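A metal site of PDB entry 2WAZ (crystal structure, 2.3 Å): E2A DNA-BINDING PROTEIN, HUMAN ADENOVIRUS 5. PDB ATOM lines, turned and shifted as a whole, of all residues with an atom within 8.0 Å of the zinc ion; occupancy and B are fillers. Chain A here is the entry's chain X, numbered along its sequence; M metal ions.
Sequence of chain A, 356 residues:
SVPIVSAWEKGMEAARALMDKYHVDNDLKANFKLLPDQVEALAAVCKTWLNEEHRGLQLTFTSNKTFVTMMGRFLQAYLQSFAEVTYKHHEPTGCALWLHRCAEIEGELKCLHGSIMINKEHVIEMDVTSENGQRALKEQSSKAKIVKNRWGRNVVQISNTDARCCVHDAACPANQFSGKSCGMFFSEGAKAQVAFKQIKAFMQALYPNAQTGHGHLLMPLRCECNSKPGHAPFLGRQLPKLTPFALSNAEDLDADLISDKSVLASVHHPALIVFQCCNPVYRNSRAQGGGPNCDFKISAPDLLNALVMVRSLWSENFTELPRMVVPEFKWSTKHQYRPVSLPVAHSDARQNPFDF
The side-chain sulfur of Cys 277 lies close to the backbone NH of Asn 279, 3.3 Å away. The backbone NH (N) of Cys 277 lies within hydrogen-bond range of the backbone carbonyl oxygen (O) of Phe 296, 3.5 Å away. The backbone carbonyl oxygen of Cys 277 sits at hydrogen-bond distance from the backbone NH of Lys 241, at 3.1 Å. The side-chain sulfur of Cys 225 sits close to the backbone NH of Asn 293 (3.8 Å). The side-chain sulfur (SG) of Cys 294 sits close to the backbone NH (N) of Glu 224, 3.6 Å away. The backbone NH (N) of Phe 296 lies close to the side-chain sulfur (SG) of Cys 294, 3.7 Å away. The side-chain sulfur of Cys 223 sits close to the backbone NH of Cys 278, at 3.5 Å. The backbone carbonyl oxygen (O) of Leu 239 sits close to the side-chain sulfur (SG) of Cys 278, 3.5 Å away.
Residues that only touch the zinc ion: Cys 278 (3.9 Å). Of the 20 residues printed, 5 come within 4 Å of the zinc ion.
The zinc ion is bound by the side-chain sulfur (SG) of Cys 277 (2.3 Å), the side-chain sulfur (SG) of Cys 225 (2.3 Å), the side-chain sulfur (SG) of Cys 294 (2.3 Å) and the side-chain sulfur (SG) of Cys 223 (2.3 Å).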
ATOM      1  N   ARG A 222      -0.736 -16.794   9.142  1.00  0.00           N
ATOM      2  CA  ARG A 222      -0.123 -15.840  10.101  1.00  0.00           C
ATOM      3  C   ARG A 222      -1.141 -15.237  11.058  1.00  0.00           C
ATOM      4  O   ARG A 222      -2.240 -14.898  10.686  1.00  0.00           O
ATOM      5  CB  ARG A 222       0.541 -14.740   9.339  1.00  0.00           C
ATOM      6  CG  ARG A 222       1.449 -15.232   8.173  1.00  0.00           C
ATOM      7  CD  ARG A 222       2.400 -14.099   7.625  1.00  0.00           C
ATOM      8  NE  ARG A 222       1.696 -12.928   7.109  1.00  0.00           N
ATOM      9  CZ  ARG A 222       1.587 -12.642   5.799  1.00  0.00           C
ATOM     10  NH1 ARG A 222       2.145 -13.437   4.848  1.00  0.00           N
ATOM     11  NH2 ARG A 222       0.964 -11.526   5.441  1.00  0.00           N
ATOM     12  N   CYS A 223      -0.789 -15.181  12.330  1.00  0.00           N
ATOM     13  CA  CYS A 223      -1.613 -14.466  13.285  1.00  0.00           C
ATOM     14  C   CYS A 223      -0.777 -13.172  13.505  1.00  0.00           C
ATOM     15  O   CYS A 223       0.148 -12.915  12.715  1.00  0.00           O
ATOM     16  CB  CYS A 223      -1.794 -15.323  14.558  1.00  0.00           C
ATOM     17  SG  CYS A 223      -0.238 -15.710  15.467  1.00  0.00           S
ATOM     18  N   GLU A 224      -1.049 -12.392  14.545  1.00  0.00           N
ATOM     19  CA  GLU A 224      -0.190 -11.208  14.855  1.00  0.00           C
ATOM     20  C   GLU A 224       1.266 -11.622  15.154  1.00  0.00           C
ATOM     21  O   GLU A 224       2.195 -10.973  14.680  1.00  0.00           O
ATOM     22  CB  GLU A 224      -0.803 -10.388  16.014  1.00  0.00           C
ATOM     23  CG  GLU A 224      -2.380 -10.257  15.878  1.00  0.00           C
ATOM     24  CD  GLU A 224      -3.129  -9.363  16.931  1.00  0.00           C
ATOM     25  OE1 GLU A 224      -2.578  -8.375  17.502  1.00  0.00           O
ATOM     26  OE2 GLU A 224      -4.356  -9.639  17.129  1.00  0.00           O
ATOM     27  N   CYS A 225       1.438 -12.736  15.891  1.00  0.00           N
ATOM     28  CA  CYS A 225       2.766 -13.187  16.347  1.00  0.00           C
ATOM     29  C   CYS A 225       3.765 -13.345  15.202  1.00  0.00           C
ATOM     30  O   CYS A 225       4.949 -13.020  15.361  1.00  0.00           O
ATOM     31  CB  CYS A 225       2.677 -14.480  17.169  1.00  0.00           C
ATOM     32  SG  CYS A 225       1.529 -14.444  18.564  1.00  0.00           S
ATOM     33  N   ASN A 226       3.313 -13.863  14.045  1.00  0.00           N
ATOM     34  CA  ASN A 226       4.208 -14.022  12.912  1.00  0.00           C
ATOM     35  C   ASN A 226       3.773 -13.252  11.688  1.00  0.00           C
ATOM     36  O   ASN A 226       4.103 -13.623  10.559  1.00  0.00           O
ATOM     37  CB  ASN A 226       4.478 -15.512  12.563  1.00  0.00           C
ATOM     38  CG  ASN A 226       3.194 -16.288  12.213  1.00  0.00           C
ATOM     39  OD1 ASN A 226       2.099 -15.849  12.480  1.00  0.00           O
ATOM     40  ND2 ASN A 226       3.355 -17.468  11.660  1.00  0.00           N
ATOM     41  N   SER A 227       3.064 -12.160  11.873  1.00  0.00           N
ATOM     42  CA  SER A 227       2.663 -11.410  10.647  1.00  0.00           C
ATOM     43  C   SER A 227       3.832 -10.775   9.868  1.00  0.00           C
ATOM     44  O   SER A 227       3.696 -10.529   8.680  1.00  0.00           O
ATOM     45  CB  SER A 227       1.578 -10.356  10.920  1.00  0.00           C
ATOM     46  OG  SER A 227       2.168  -9.369  11.762  1.00  0.00           O
ATOM     47  N   PHE A 234       9.818 -18.138  17.597  1.00  0.00           N
ATOM     48  CA  PHE A 234       9.119 -18.625  18.783  1.00  0.00           C
ATOM     49  C   PHE A 234       8.874 -20.125  18.631  1.00  0.00           C
ATOM     50  O   PHE A 234       8.886 -20.707  17.524  1.00  0.00           O
ATOM     51  CB  PHE A 234       7.807 -17.848  19.121  1.00  0.00           C
ATOM     52  CG  PHE A 234       6.800 -17.791  17.992  1.00  0.00           C
ATOM     53  CD1 PHE A 234       5.929 -18.863  17.738  1.00  0.00           C
ATOM     54  CD2 PHE A 234       6.717 -16.636  17.178  1.00  0.00           C
ATOM     55  CE1 PHE A 234       4.990 -18.813  16.664  1.00  0.00           C
ATOM     56  CE2 PHE A 234       5.777 -16.547  16.093  1.00  0.00           C
ATOM     57  CZ  PHE A 234       4.898 -17.654  15.851  1.00  0.00           C
ATOM     58  N   LEU A 239       1.715 -21.956  12.828  1.00  0.00           N
ATOM     59  CA  LEU A 239       0.598 -21.523  12.013  1.00  0.00           C
ATOM     60  C   LEU A 239      -0.555 -21.291  12.958  1.00  0.00           C
ATOM     61  O   LEU A 239      -0.587 -21.933  14.034  1.00  0.00           O
ATOM     62  CB  LEU A 239       0.198 -22.646  11.031  1.00  0.00           C
ATOM     63  CG  LEU A 239       1.239 -22.756   9.930  1.00  0.00           C
ATOM     64  CD1 LEU A 239       0.980 -23.948   9.066  1.00  0.00           C
ATOM     65  CD2 LEU A 239       1.195 -21.434   9.116  1.00  0.00           C
ATOM     66  N   PRO A 240      -1.524 -20.410  12.594  1.00  0.00           N
ATOM     67  CA  PRO A 240      -2.720 -20.240  13.420  1.00  0.00           C
ATOM     68  C   PRO A 240      -3.369 -21.594  13.807  1.00  0.00           C
ATOM     69  O   PRO A 240      -3.569 -22.444  12.922  1.00  0.00           O
ATOM     70  CB  PRO A 240      -3.657 -19.484  12.475  1.00  0.00           C
ATOM     71  CG  PRO A 240      -2.631 -18.489  11.787  1.00  0.00           C
ATOM     72  CD  PRO A 240      -1.500 -19.419  11.484  1.00  0.00           C
ATOM     73  N   LYS A 241      -3.688 -21.795  15.085  1.00  0.00           N
ATOM     74  CA  LYS A 241      -4.351 -23.055  15.502  1.00  0.00           C
ATOM     75  C   LYS A 241      -5.733 -23.213  14.853  1.00  0.00           C
ATOM     76  O   LYS A 241      -6.462 -22.239  14.681  1.00  0.00           O
ATOM     77  CB  LYS A 241      -4.465 -23.109  17.023  1.00  0.00           C
ATOM     78  CG  LYS A 241      -4.932 -24.465  17.587  1.00  0.00           C
ATOM     79  CD  LYS A 241      -5.069 -24.320  19.131  1.00  0.00           C
ATOM     80  CE  LYS A 241      -5.003 -25.696  19.873  1.00  0.00           C
ATOM     81  NZ  LYS A 241      -6.263 -26.449  19.694  1.00  0.00           N
ATOM     82  N   GLN A 276      -7.204 -19.500  15.525  1.00  0.00           N
ATOM     83  CA  GLN A 276      -6.730 -18.637  16.597  1.00  0.00           C
ATOM     84  C   GLN A 276      -5.212 -18.400  16.431  1.00  0.00           C
ATOM     85  O   GLN A 276      -4.602 -18.783  15.433  1.00  0.00           O
ATOM     86  CB  GLN A 276      -7.121 -19.194  18.025  1.00  0.00           C
ATOM     87  CG  GLN A 276      -8.648 -19.207  18.179  1.00  0.00           C
ATOM     88  CD  GLN A 276      -9.136 -20.010  19.401  1.00  0.00           C
ATOM     89  OE1 GLN A 276      -9.508 -19.422  20.443  1.00  0.00           O
ATOM     90  NE2 GLN A 276      -9.136 -21.331  19.288  1.00  0.00           N
ATOM     91  N   CYS A 277      -4.631 -17.722  17.418  1.00  0.00           N
ATOM     92  CA  CYS A 277      -3.183 -17.532  17.494  1.00  0.00           C
ATOM     93  C   CYS A 277      -2.443 -18.877  17.202  1.00  0.00           C
ATOM     94  O   CYS A 277      -3.003 -19.941  17.424  1.00  0.00           O
ATOM     95  CB  CYS A 277      -2.843 -17.011  18.890  1.00  0.00           C
ATOM     96  SG  CYS A 277      -1.057 -16.855  19.137  1.00  0.00           S
ATOM     97  N   CYS A 278      -1.215 -18.826  16.685  1.00  0.00           N
ATOM     98  CA  CYS A 278      -0.374 -20.040  16.615  1.00  0.00           C
ATOM     99  C   CYS A 278      -0.339 -20.777  17.983  1.00  0.00           C
ATOM    100  O   CYS A 278      -0.464 -22.013  18.054  1.00  0.00           O
ATOM    101  CB  CYS A 278       1.077 -19.694  16.192  1.00  0.00           C
ATOM    102  SG  CYS A 278       1.149 -18.925  14.552  1.00  0.00           S
ATOM    103  N   ASN A 279      -0.143 -20.013  19.064  1.00  0.00           N
ATOM    104  CA  ASN A 279      -0.103 -20.599  20.394  1.00  0.00           C
ATOM    105  C   ASN A 279      -1.078 -19.903  21.354  1.00  0.00           C
ATOM    106  O   ASN A 279      -0.683 -19.004  22.110  1.00  0.00           O
ATOM    107  CB  ASN A 279       1.320 -20.635  20.920  1.00  0.00           C
ATOM    108  CG  ASN A 279       2.254 -21.281  19.957  1.00  0.00           C
ATOM    109  OD1 ASN A 279       2.911 -20.590  19.174  1.00  0.00           O
ATOM    110  ND2 ASN A 279       2.280 -22.607  19.937  1.00  0.00           N
ATOM    111  N   PRO A 280      -2.367 -20.298  21.285  1.00  0.00           N
ATOM    112  CA  PRO A 280      -3.377 -19.546  22.071  1.00  0.00           C
ATOM    113  C   PRO A 280      -3.209 -19.867  23.552  1.00  0.00           C
ATOM    114  O   PRO A 280      -2.785 -20.989  23.935  1.00  0.00           O
ATOM    115  CB  PRO A 280      -4.752 -20.021  21.514  1.00  0.00           C
ATOM    116  CG  PRO A 280      -4.408 -20.894  20.263  1.00  0.00           C
ATOM    117  CD  PRO A 280      -2.966 -21.385  20.482  1.00  0.00           C
ATOM    118  N   PRO A 292       5.273 -15.381  22.693  1.00  0.00           N
ATOM    119  CA  PRO A 292       4.190 -14.454  22.279  1.00  0.00           C
ATOM    120  C   PRO A 292       2.842 -15.160  22.125  1.00  0.00           C
ATOM    121  O   PRO A 292       2.781 -16.375  21.887  1.00  0.00           O
ATOM    122  CB  PRO A 292       4.658 -13.948  20.917  1.00  0.00           C
ATOM    123  CG  PRO A 292       5.503 -15.089  20.391  1.00  0.00           C
ATOM    124  CD  PRO A 292       6.186 -15.709  21.574  1.00  0.00           C
ATOM    125  N   ASN A 293       1.772 -14.414  22.350  1.00  0.00           N
ATOM    126  CA  ASN A 293       0.430 -14.892  22.001  1.00  0.00           C
ATOM    127  C   ASN A 293      -0.503 -13.719  21.716  1.00  0.00           C
ATOM    128  O   ASN A 293      -0.268 -12.630  22.216  1.00  0.00           O
ATOM    129  CB  ASN A 293      -0.133 -15.789  23.073  1.00  0.00           C
ATOM    130  CG  ASN A 293      -0.433 -15.040  24.331  1.00  0.00           C
ATOM    131  OD1 ASN A 293       0.388 -14.994  25.223  1.00  0.00           O
ATOM    132  ND2 ASN A 293      -1.609 -14.441  24.412  1.00  0.00           N
ATOM    133  N   CYS A 294      -1.574 -13.948  20.949  1.00  0.00           N
ATOM    134  CA  CYS A 294      -2.388 -12.811  20.490  1.00  0.00           C
ATOM    135  C   CYS A 294      -3.876 -13.160  20.519  1.00  0.00           C
ATOM    136  O   CYS A 294      -4.277 -14.277  20.803  1.00  0.00           O
ATOM    137  CB  CYS A 294      -1.921 -12.346  19.108  1.00  0.00           C
ATOM    138  SG  CYS A 294      -2.257 -13.518  17.719  1.00  0.00           S
ATOM    139  N   ASP A 295      -4.702 -12.164  20.253  1.00  0.00           N
ATOM    140  CA  ASP A 295      -6.131 -12.376  20.308  1.00  0.00           C
ATOM    141  C   ASP A 295      -6.731 -12.724  18.891  1.00  0.00           C
ATOM    142  O   ASP A 295      -7.944 -12.637  18.689  1.00  0.00           O
ATOM    143  CB  ASP A 295      -6.812 -11.123  20.943  1.00  0.00           C
ATOM    144  CG  ASP A 295      -6.345  -9.775  20.274  1.00  0.00           C
ATOM    145  OD1 ASP A 295      -5.783  -9.827  19.131  1.00  0.00           O
ATOM    146  OD2 ASP A 295      -6.553  -8.658  20.851  1.00  0.00           O
ATOM    147  N   PHE A 296      -5.879 -13.092  17.923  1.00  0.00           N
ATOM    148  CA  PHE A 296      -6.380 -13.378  16.589  1.00  0.00           C
ATOM    149  C   PHE A 296      -7.486 -14.450  16.678  1.00  0.00           C
ATOM    150  O   PHE A 296      -7.251 -15.481  17.273  1.00  0.00           O
ATOM    151  CB  PHE A 296      -5.230 -13.864  15.750  1.00  0.00           C
ATOM    152  CG  PHE A 296      -5.584 -14.211  14.361  1.00  0.00           C
ATOM    153  CD1 PHE A 296      -5.406 -13.265  13.344  1.00  0.00           C
ATOM    154  CD2 PHE A 296      -6.007 -15.523  14.044  1.00  0.00           C
ATOM    155  CE1 PHE A 296      -5.724 -13.574  11.998  1.00  0.00           C
ATOM    156  CE2 PHE A 296      -6.305 -15.874  12.679  1.00  0.00           C
ATOM    157  CZ  PHE A 296      -6.150 -14.887  11.649  1.00  0.00           C
HETATM  158 ZN    ZN M   1      -0.546 -15.115  17.717  1.00  0.00          ZN
